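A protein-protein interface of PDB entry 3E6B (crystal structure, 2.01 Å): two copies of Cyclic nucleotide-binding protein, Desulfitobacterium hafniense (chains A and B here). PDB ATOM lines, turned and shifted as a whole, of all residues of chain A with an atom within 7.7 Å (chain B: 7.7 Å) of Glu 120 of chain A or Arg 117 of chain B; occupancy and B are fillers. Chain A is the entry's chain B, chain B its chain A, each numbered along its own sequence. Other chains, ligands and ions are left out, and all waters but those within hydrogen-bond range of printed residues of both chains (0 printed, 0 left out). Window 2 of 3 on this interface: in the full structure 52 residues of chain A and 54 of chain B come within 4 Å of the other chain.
Among the printed residues, pairs that only touch across the chains: Ile 123 of chain A with Ile 123 of chain B, Phe 124 of chain A with Glu 109 of chain B, Phe 116 of chain A with Ile 123 of chain B, Phe 124 of chain A with Phe 116 of chain B, Phe 124 of chain A with Arg 113 of chain B, Ile 123 of chain A with Phe 116 of chain B and Phe 124 of chain A with Leu 112 of chain B.
Val 115 of chain A touches none of the printed residues of chain B. Printed residues of chain B within 4 Å of Phe 116 of chain A: Ile 123 (3.7 Å). Of the printed residues of chain B, Glu 120 of chain A touches Arg 113 and Arg 117. Of the printed residues of chain B, Phe 124 of chain A touches Glu 109, Leu 112, Arg 113 and Phe 116. Printed residues of chain A within 4 Å of Glu 109 of chain B: Phe 124 (3.7 Å). Printed residues of chain A within 4 Å of Leu 112 of chain B: Phe 124. Of the printed residues of chain A, Arg 113 of chain B touches Glu 120 (2.8 Å), Asp 121 (2.8 Å) and Phe 124 (3.8 Å). Arg 117 of chain B touches one residue of chain A. Met 122 of chain B touches none of the printed residues of chain A. The nearest printed residue of chain A that does not touch Arg 113 of chain B is Met 122 of chain A (6.7 Å).
Printed residues of chain B that touch a printed residue of chain A: Glu 109, Leu 112, Arg 113, Phe 116, Arg 117, Glu 120 and Ile 123. Along chain B the printed residues that touch a printed residue of chain A span positions 109 to 123. Printed residues of chain A that touch a printed residue of chain B: Phe 116, Arg 117, Glu 120, Asp 121, Ile 123 and Phe 124. Hydrophobic or aromatic side chains of chain A that line the printed part of chain B: Phe 116, Ile 123 and Phe 124. Among the printed residues, 11 pairs touch across the chains. Among the printed residues, Asp or Glu carboxylates within 4 Å of a Lys or Arg side-chain nitrogen of the other chain: Arg 117 of chain A with Glu 120 of chain B, Glu 120 of chain A with Arg 113 of chain B, Glu 120 of chain A with Arg 117 of chain B and Asp 121 of chain A with Arg 113 of chain B.
Phe 116 of chain A touches Ile 123 of chain B, and with the chains exchanged Ile 123 of chain A touches Phe 116 of chain B. Arg 117 of chain A touches Glu 120 of chain B, and with the chains exchanged Glu 120 of chain A touches Arg 117 of chain B. Ile 123 of chain B touches its own counterpart, Ile 123 of chain A. 8 positions are printed for both chains. Of the 11 pairs that touch across the chains among the printed residues, 5 have their exchanged pair printed and touching as well.
The side-chain carboxylate (OD1) of Asp 121 of chain A lies within salt-bridge range of the guanidinium group (NH2) of Arg 113 of chain B (2.8 Å). OE2 of Glu 120 of chain A is in salt-bridge range of NE of Arg 117 of chain B (2.7 Å). OE1 of Glu 120 of chain A is in salt-bridge range of NH1 of Arg 113 of chain B, 2.8 Å away. The side-chain carboxylate of Glu 120 of chain B lies within salt-bridge range of the guanidinium group of Arg 117 of chain A (2.8 Å).
OD2 of Asp 119 of chain A sits at hydrogen-bond distance from N of Asp 121 of chain A. The guanidinium group (NH2) of Arg 113 of chain B lies within salt-bridge range of the side-chain carboxylate (OE2) of Glu 109 of chain B (3.4 Å).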
ATOM      1  N   TYR A  28     -21.599   1.213  -4.967  1.00  0.00           N
ATOM      2  CA  TYR A  28     -20.647   1.756  -5.954  1.00  0.00           C
ATOM      3  C   TYR A  28     -20.974   1.446  -7.395  1.00  0.00           C
ATOM      4  O   TYR A  28     -20.121   1.681  -8.282  1.00  0.00           O
ATOM      5  CB  TYR A  28     -19.168   1.359  -5.623  1.00  0.00           C
ATOM      6  CG  TYR A  28     -18.782   1.680  -4.202  1.00  0.00           C
ATOM      7  CD1 TYR A  28     -18.592   0.694  -3.292  1.00  0.00           C
ATOM      8  CD2 TYR A  28     -18.668   3.000  -3.757  1.00  0.00           C
ATOM      9  CE1 TYR A  28     -18.301   0.970  -1.985  1.00  0.00           C
ATOM     10  CE2 TYR A  28     -18.357   3.277  -2.414  1.00  0.00           C
ATOM     11  CZ  TYR A  28     -18.151   2.277  -1.546  1.00  0.00           C
ATOM     12  OH  TYR A  28     -17.832   2.494  -0.183  1.00  0.00           O
ATOM     13  N   VAL A 115     -13.532   3.120  -7.852  1.00  0.00           N
ATOM     14  CA  VAL A 115     -14.101   2.537  -6.608  1.00  0.00           C
ATOM     15  C   VAL A 115     -13.068   2.591  -5.475  1.00  0.00           C
ATOM     16  O   VAL A 115     -13.363   3.057  -4.356  1.00  0.00           O
ATOM     17  CB  VAL A 115     -14.613   1.053  -6.816  1.00  0.00           C
ATOM     18  CG1 VAL A 115     -15.034   0.444  -5.465  1.00  0.00           C
ATOM     19  CG2 VAL A 115     -15.769   0.990  -7.896  1.00  0.00           C
ATOM     20  N   PHE A 116     -11.868   2.053  -5.714  1.00  0.00           N
ATOM     21  CA  PHE A 116     -10.869   2.009  -4.622  1.00  0.00           C
ATOM     22  C   PHE A 116     -10.438   3.374  -4.102  1.00  0.00           C
ATOM     23  O   PHE A 116     -10.125   3.469  -2.957  1.00  0.00           O
ATOM     24  CB  PHE A 116      -9.637   1.171  -4.980  1.00  0.00           C
ATOM     25  CG  PHE A 116      -9.980  -0.198  -5.503  1.00  0.00           C
ATOM     26  CD1 PHE A 116     -11.102  -0.876  -5.036  1.00  0.00           C
ATOM     27  CD2 PHE A 116      -9.217  -0.784  -6.495  1.00  0.00           C
ATOM     28  CE1 PHE A 116     -11.420  -2.158  -5.534  1.00  0.00           C
ATOM     29  CE2 PHE A 116      -9.526  -2.040  -6.987  1.00  0.00           C
ATOM     30  CZ  PHE A 116     -10.641  -2.721  -6.519  1.00  0.00           C
ATOM     31  N   ARG A 117     -10.369   4.395  -4.982  1.00  0.00           N
ATOM     32  CA  ARG A 117     -10.092   5.803  -4.573  1.00  0.00           C
ATOM     33  C   ARG A 117     -11.142   6.370  -3.613  1.00  0.00           C
ATOM     34  O   ARG A 117     -10.844   7.225  -2.785  1.00  0.00           O
ATOM     35  CB  ARG A 117      -9.911   6.700  -5.820  1.00  0.00           C
ATOM     36  CG  ARG A 117      -8.628   6.244  -6.572  1.00  0.00           C
ATOM     37  CD  ARG A 117      -8.439   6.964  -7.851  1.00  0.00           C
ATOM     38  NE  ARG A 117      -7.365   6.295  -8.582  1.00  0.00           N
ATOM     39  CZ  ARG A 117      -6.920   6.705  -9.755  1.00  0.00           C
ATOM     40  NH1 ARG A 117      -7.484   7.761 -10.321  1.00  0.00           N
ATOM     41  NH2 ARG A 117      -5.923   6.056 -10.350  1.00  0.00           N
ATOM     42  N   THR A 118     -12.356   5.865  -3.729  1.00  0.00           N
ATOM     43  CA  THR A 118     -13.442   6.213  -2.791  1.00  0.00           C
ATOM     44  C   THR A 118     -13.492   5.401  -1.525  1.00  0.00           C
ATOM     45  O   THR A 118     -13.830   5.901  -0.449  1.00  0.00           O
ATOM     46  CB  THR A 118     -14.797   6.133  -3.565  1.00  0.00           C
ATOM     47  OG1 THR A 118     -14.834   7.229  -4.495  1.00  0.00           O
ATOM     48  CG2 THR A 118     -15.976   6.255  -2.618  1.00  0.00           C
ATOM     49  N   ASP A 119     -13.155   4.124  -1.622  1.00  0.00           N
ATOM     50  CA  ASP A 119     -13.213   3.268  -0.482  1.00  0.00           C
ATOM     51  C   ASP A 119     -12.170   2.167  -0.663  1.00  0.00           C
ATOM     52  O   ASP A 119     -12.374   1.161  -1.436  1.00  0.00           O
ATOM     53  CB  ASP A 119     -14.647   2.680  -0.334  1.00  0.00           C
ATOM     54  CG  ASP A 119     -14.782   1.812   0.876  1.00  0.00           C
ATOM     55  OD1 ASP A 119     -15.853   1.227   1.048  1.00  0.00           O
ATOM     56  OD2 ASP A 119     -13.819   1.695   1.684  1.00  0.00           O
ATOM     57  N   GLU A 120     -11.085   2.344   0.083  1.00  0.00           N
ATOM     58  CA  GLU A 120      -9.916   1.478   0.029  1.00  0.00           C
ATOM     59  C   GLU A 120     -10.298   0.072   0.505  1.00  0.00           C
ATOM     60  O   GLU A 120      -9.658  -0.903   0.157  1.00  0.00           O
ATOM     61  CB  GLU A 120      -8.833   2.058   0.953  1.00  0.00           C
ATOM     62  CG  GLU A 120      -7.467   1.327   0.969  1.00  0.00           C
ATOM     63  CD  GLU A 120      -6.469   2.002   1.966  1.00  0.00           C
ATOM     64  OE1 GLU A 120      -6.511   1.699   3.202  1.00  0.00           O
ATOM     65  OE2 GLU A 120      -5.611   2.821   1.480  1.00  0.00           O
ATOM     66  N   ASP A 121     -11.293  -0.032   1.386  1.00  0.00           N
ATOM     67  CA  ASP A 121     -11.682  -1.372   1.902  1.00  0.00           C
ATOM     68  C   ASP A 121     -12.240  -2.291   0.815  1.00  0.00           C
ATOM     69  O   ASP A 121     -12.159  -3.519   0.972  1.00  0.00           O
ATOM     70  CB  ASP A 121     -12.699  -1.272   3.049  1.00  0.00           C
ATOM     71  CG  ASP A 121     -12.067  -0.943   4.374  1.00  0.00           C
ATOM     72  OD1 ASP A 121     -10.796  -0.891   4.538  1.00  0.00           O
ATOM     73  OD2 ASP A 121     -12.900  -0.801   5.311  1.00  0.00           O
ATOM     74  N   MET A 122     -12.725  -1.749  -0.316  1.00  0.00           N
ATOM     75  CA  MET A 122     -13.278  -2.624  -1.374  1.00  0.00           C
ATOM     76  C   MET A 122     -12.183  -3.470  -2.014  1.00  0.00           C
ATOM     77  O   MET A 122     -12.442  -4.532  -2.617  1.00  0.00           O
ATOM     78  CB  MET A 122     -13.995  -1.813  -2.443  1.00  0.00           C
ATOM     79  CG  MET A 122     -15.300  -1.105  -1.958  1.00  0.00           C
ATOM     80  SD  MET A 122     -16.506  -2.345  -1.234  1.00  0.00           S
ATOM     81  CE  MET A 122     -16.082  -2.257   0.507  1.00  0.00           C
ATOM     82  N   ILE A 123     -10.937  -3.029  -1.879  1.00  0.00           N
ATOM     83  CA  ILE A 123      -9.806  -3.854  -2.382  1.00  0.00           C
ATOM     84  C   ILE A 123      -9.820  -5.189  -1.659  1.00  0.00           C
ATOM     85  O   ILE A 123      -9.658  -6.244  -2.262  1.00  0.00           O
ATOM     86  CB  ILE A 123      -8.417  -3.163  -2.113  1.00  0.00           C
ATOM     87  CG1 ILE A 123      -8.221  -1.893  -2.993  1.00  0.00           C
ATOM     88  CG2 ILE A 123      -7.245  -4.187  -2.208  1.00  0.00           C
ATOM     89  CD1 ILE A 123      -7.115  -0.931  -2.382  1.00  0.00           C
ATOM     90  N   PHE A 124      -9.963  -5.123  -0.343  1.00  0.00           N
ATOM     91  CA  PHE A 124      -9.787  -6.294   0.553  1.00  0.00           C
ATOM     92  C   PHE A 124     -10.999  -7.204   0.556  1.00  0.00           C
ATOM     93  O   PHE A 124     -10.857  -8.408   0.696  1.00  0.00           O
ATOM     94  CB  PHE A 124      -9.439  -5.820   1.981  1.00  0.00           C
ATOM     95  CG  PHE A 124      -8.061  -5.153   2.037  1.00  0.00           C
ATOM     96  CD1 PHE A 124      -6.921  -5.925   2.093  1.00  0.00           C
ATOM     97  CD2 PHE A 124      -7.939  -3.775   1.887  1.00  0.00           C
ATOM     98  CE1 PHE A 124      -5.634  -5.337   2.059  1.00  0.00           C
ATOM     99  CE2 PHE A 124      -6.695  -3.177   1.813  1.00  0.00           C
ATOM    100  CZ  PHE A 124      -5.536  -3.957   1.926  1.00  0.00           C
ATOM    101  N   GLU A 125     -12.168  -6.603   0.356  1.00  0.00           N
ATOM    102  CA  GLU A 125     -13.420  -7.352   0.083  1.00  0.00           C
ATOM    103  C   GLU A 125     -13.273  -8.219  -1.158  1.00  0.00           C
ATOM    104  O   GLU A 125     -13.690  -9.378  -1.185  1.00  0.00           O
ATOM    105  CB  GLU A 125     -14.592  -6.379  -0.086  1.00  0.00           C
ATOM    106  CG  GLU A 125     -14.872  -5.603   1.183  1.00  0.00           C
ATOM    107  CD  GLU A 125     -15.315  -6.509   2.342  1.00  0.00           C
ATOM    108  OE1 GLU A 125     -16.435  -7.051   2.256  1.00  0.00           O
ATOM    109  OE2 GLU A 125     -14.562  -6.673   3.343  1.00  0.00           O
ATOM    110  N   MET B  31       8.371  -2.896   3.142  1.00  0.00           N
ATOM    111  CA  MET B  31       7.095  -2.552   3.815  1.00  0.00           C
ATOM    112  C   MET B  31       6.428  -3.709   4.579  1.00  0.00           C
ATOM    113  O   MET B  31       5.405  -3.495   5.245  1.00  0.00           O
ATOM    114  CB  MET B  31       6.127  -1.922   2.812  1.00  0.00           C
ATOM    115  CG  MET B  31       6.717  -0.669   2.162  1.00  0.00           C
ATOM    116  SD  MET B  31       5.850   0.031   0.753  1.00  0.00           S
ATOM    117  CE  MET B  31       6.906   1.412   0.312  1.00  0.00           C
ATOM    118  N   GLU B 109      -2.475  -7.047   6.454  1.00  0.00           N
ATOM    119  CA  GLU B 109      -3.409  -6.100   5.808  1.00  0.00           C
ATOM    120  C   GLU B 109      -2.930  -4.627   5.852  1.00  0.00           C
ATOM    121  O   GLU B 109      -3.014  -3.903   4.845  1.00  0.00           O
ATOM    122  CB  GLU B 109      -4.786  -6.232   6.436  1.00  0.00           C
ATOM    123  CG  GLU B 109      -5.869  -5.482   5.715  1.00  0.00           C
ATOM    124  CD  GLU B 109      -7.172  -5.522   6.471  1.00  0.00           C
ATOM    125  OE1 GLU B 109      -8.071  -6.357   6.154  1.00  0.00           O
ATOM    126  OE2 GLU B 109      -7.277  -4.710   7.395  1.00  0.00           O
ATOM    127  N   LYS B 110      -2.434  -4.220   7.017  1.00  0.00           N
ATOM    128  CA  LYS B 110      -1.853  -2.897   7.291  1.00  0.00           C
ATOM    129  C   LYS B 110      -0.693  -2.558   6.324  1.00  0.00           C
ATOM    130  O   LYS B 110      -0.710  -1.515   5.644  1.00  0.00           O
ATOM    131  CB  LYS B 110      -1.407  -2.864   8.767  1.00  0.00           C
ATOM    132  CG  LYS B 110      -1.174  -1.470   9.364  1.00  0.00           C
ATOM    133  CD  LYS B 110      -0.764  -1.557  10.875  1.00  0.00           C
ATOM    134  CE  LYS B 110       0.548  -0.729  11.160  1.00  0.00           C
ATOM    135  NZ  LYS B 110       0.505   0.690  10.571  1.00  0.00           N
ATOM    136  N   SER B 111       0.275  -3.454   6.204  1.00  0.00           N
ATOM    137  CA  SER B 111       1.378  -3.254   5.308  1.00  0.00           C
ATOM    138  C   SER B 111       0.990  -3.275   3.799  1.00  0.00           C
ATOM    139  O   SER B 111       1.519  -2.471   2.994  1.00  0.00           O
ATOM    140  CB  SER B 111       2.523  -4.237   5.680  1.00  0.00           C
ATOM    141  OG  SER B 111       2.423  -5.362   4.845  1.00  0.00           O
ATOM    142  N   LEU B 112       0.027  -4.120   3.402  1.00  0.00           N
ATOM    143  CA  LEU B 112      -0.555  -4.022   2.037  1.00  0.00           C
ATOM    144  C   LEU B 112      -1.176  -2.647   1.771  1.00  0.00           C
ATOM    145  O   LEU B 112      -1.016  -2.136   0.664  1.00  0.00           O
ATOM    146  CB  LEU B 112      -1.623  -5.110   1.800  1.00  0.00           C
ATOM    147  CG  LEU B 112      -1.112  -6.552   1.824  1.00  0.00           C
ATOM    148  CD1 LEU B 112      -2.298  -7.483   1.654  1.00  0.00           C
ATOM    149  CD2 LEU B 112      -0.171  -6.700   0.667  1.00  0.00           C
ATOM    150  N   ARG B 113      -1.890  -2.048   2.745  1.00  0.00           N
ATOM    151  CA  ARG B 113      -2.439  -0.681   2.540  1.00  0.00           C
ATOM    152  C   ARG B 113      -1.267   0.278   2.186  1.00  0.00           C
ATOM    153  O   ARG B 113      -1.385   1.091   1.271  1.00  0.00           O
ATOM    154  CB  ARG B 113      -3.184  -0.152   3.776  1.00  0.00           C
ATOM    155  CG  ARG B 113      -4.358  -1.077   4.170  1.00  0.00           C
ATOM    156  CD  ARG B 113      -5.313  -0.532   5.205  1.00  0.00           C
ATOM    157  NE  ARG B 113      -6.391  -1.500   5.520  1.00  0.00           N
ATOM    158  CZ  ARG B 113      -7.647  -1.415   5.056  1.00  0.00           C
ATOM    159  NH1 ARG B 113      -8.002  -0.438   4.230  1.00  0.00           N
ATOM    160  NH2 ARG B 113      -8.570  -2.323   5.389  1.00  0.00           N
ATOM    161  N   THR B 114      -0.177   0.199   2.940  1.00  0.00           N
ATOM    162  CA  THR B 114       1.023   1.008   2.647  1.00  0.00           C
ATOM    163  C   THR B 114       1.538   0.758   1.225  1.00  0.00           C
ATOM    164  O   THR B 114       1.778   1.715   0.481  1.00  0.00           O
ATOM    165  CB  THR B 114       2.138   0.774   3.664  1.00  0.00           C
ATOM    166  OG1 THR B 114       1.611   1.044   4.981  1.00  0.00           O
ATOM    167  CG2 THR B 114       3.360   1.759   3.399  1.00  0.00           C
ATOM    168  N   VAL B 115       1.627  -0.510   0.802  1.00  0.00           N
ATOM    169  CA  VAL B 115       1.972  -0.811  -0.602  1.00  0.00           C
ATOM    170  C   VAL B 115       1.015  -0.137  -1.608  1.00  0.00           C
ATOM    171  O   VAL B 115       1.480   0.510  -2.574  1.00  0.00           O
ATOM    172  CB  VAL B 115       2.065  -2.355  -0.851  1.00  0.00           C
ATOM    173  CG1 VAL B 115       2.281  -2.670  -2.303  1.00  0.00           C
ATOM    174  CG2 VAL B 115       3.142  -2.955  -0.021  1.00  0.00           C
ATOM    175  N   PHE B 116      -0.325  -0.273  -1.408  1.00  0.00           N
ATOM    176  CA  PHE B 116      -1.306   0.249  -2.382  1.00  0.00           C
ATOM    177  C   PHE B 116      -1.337   1.746  -2.496  1.00  0.00           C
ATOM    178  O   PHE B 116      -1.666   2.280  -3.560  1.00  0.00           O
ATOM    179  CB  PHE B 116      -2.717  -0.297  -2.078  1.00  0.00           C
ATOM    180  CG  PHE B 116      -2.739  -1.793  -2.063  1.00  0.00           C
ATOM    181  CD1 PHE B 116      -1.870  -2.509  -2.923  1.00  0.00           C
ATOM    182  CD2 PHE B 116      -3.597  -2.509  -1.226  1.00  0.00           C
ATOM    183  CE1 PHE B 116      -1.799  -3.949  -2.883  1.00  0.00           C
ATOM    184  CE2 PHE B 116      -3.565  -3.925  -1.220  1.00  0.00           C
ATOM    185  CZ  PHE B 116      -2.663  -4.635  -2.041  1.00  0.00           C
ATOM    186  N   ARG B 117      -1.088   2.402  -1.374  1.00  0.00           N
ATOM    187  CA  ARG B 117      -1.013   3.839  -1.325  1.00  0.00           C
ATOM    188  C   ARG B 117       0.234   4.364  -2.057  1.00  0.00           C
ATOM    189  O   ARG B 117       0.208   5.454  -2.539  1.00  0.00           O
ATOM    190  CB  ARG B 117      -1.017   4.308   0.111  1.00  0.00           C
ATOM    191  CG  ARG B 117      -2.424   4.235   0.753  1.00  0.00           C
ATOM    192  CD  ARG B 117      -2.280   4.291   2.262  1.00  0.00           C
ATOM    193  NE  ARG B 117      -3.517   3.822   2.935  1.00  0.00           N
ATOM    194  CZ  ARG B 117      -3.689   3.740   4.249  1.00  0.00           C
ATOM    195  NH1 ARG B 117      -2.760   4.217   5.076  1.00  0.00           N
ATOM    196  NH2 ARG B 117      -4.857   3.307   4.739  1.00  0.00           N
ATOM    197  N   THR B 118       1.299   3.566  -2.133  1.00  0.00           N
ATOM    198  CA  THR B 118       2.540   3.871  -2.934  1.00  0.00           C
ATOM    199  C   THR B 118       2.374   3.585  -4.462  1.00  0.00           C
ATOM    200  O   THR B 118       2.704   4.408  -5.354  1.00  0.00           O
ATOM    201  CB  THR B 118       3.723   3.069  -2.310  1.00  0.00           C
ATOM    202  OG1 THR B 118       3.810   3.396  -0.914  1.00  0.00           O
ATOM    203  CG2 THR B 118       5.091   3.400  -3.023  1.00  0.00           C
ATOM    204  N   ASP B 119       1.768   2.443  -4.774  1.00  0.00           N
ATOM    205  CA  ASP B 119       1.628   1.989  -6.135  1.00  0.00           C
ATOM    206  C   ASP B 119       0.324   1.188  -6.227  1.00  0.00           C
ATOM    207  O   ASP B 119       0.216   0.023  -5.744  1.00  0.00           O
ATOM    208  CB  ASP B 119       2.848   1.119  -6.449  1.00  0.00           C
ATOM    209  CG  ASP B 119       2.832   0.511  -7.845  1.00  0.00           C
ATOM    210  OD1 ASP B 119       1.961   0.825  -8.663  1.00  0.00           O
ATOM    211  OD2 ASP B 119       3.738  -0.320  -8.119  1.00  0.00           O
ATOM    212  N   GLU B 120      -0.649   1.810  -6.857  1.00  0.00           N
ATOM    213  CA  GLU B 120      -1.980   1.279  -7.043  1.00  0.00           C
ATOM    214  C   GLU B 120      -1.999   0.061  -7.946  1.00  0.00           C
ATOM    215  O   GLU B 120      -2.909  -0.776  -7.867  1.00  0.00           O
ATOM    216  CB  GLU B 120      -2.843   2.405  -7.659  1.00  0.00           C
ATOM    217  CG  GLU B 120      -4.392   2.121  -7.725  1.00  0.00           C
ATOM    218  CD  GLU B 120      -5.140   3.302  -8.336  1.00  0.00           C
ATOM    219  OE1 GLU B 120      -5.994   3.932  -7.643  1.00  0.00           O
ATOM    220  OE2 GLU B 120      -4.837   3.606  -9.511  1.00  0.00           O
ATOM    221  N   MET B 122      -0.192  -2.430  -7.874  1.00  0.00           N
ATOM    222  CA  MET B 122      -0.004  -3.639  -7.075  1.00  0.00           C
ATOM    223  C   MET B 122      -1.329  -4.355  -6.677  1.00  0.00           C
ATOM    224  O   MET B 122      -1.329  -5.554  -6.490  1.00  0.00           O
ATOM    225  CB  MET B 122       0.886  -3.400  -5.830  1.00  0.00           C
ATOM    226  CG  MET B 122       2.363  -3.094  -6.147  1.00  0.00           C
ATOM    227  SD  MET B 122       3.131  -4.396  -7.165  1.00  0.00           S
ATOM    228  CE  MET B 122       2.995  -3.684  -8.758  1.00  0.00           C
ATOM    229  N   ILE B 123      -2.414  -3.611  -6.522  1.00  0.00           N
ATOM    230  CA  ILE B 123      -3.747  -4.186  -6.213  1.00  0.00           C
ATOM    231  C   ILE B 123      -4.091  -5.178  -7.325  1.00  0.00           C
ATOM    232  O   ILE B 123      -4.514  -6.297  -7.057  1.00  0.00           O
ATOM    233  CB  ILE B 123      -4.818  -3.078  -6.238  1.00  0.00           C
ATOM    234  CG1 ILE B 123      -4.615  -2.083  -5.078  1.00  0.00           C
ATOM    235  CG2 ILE B 123      -6.305  -3.702  -6.272  1.00  0.00           C
ATOM    236  CD1 ILE B 123      -5.318  -0.710  -5.348  1.00  0.00           C
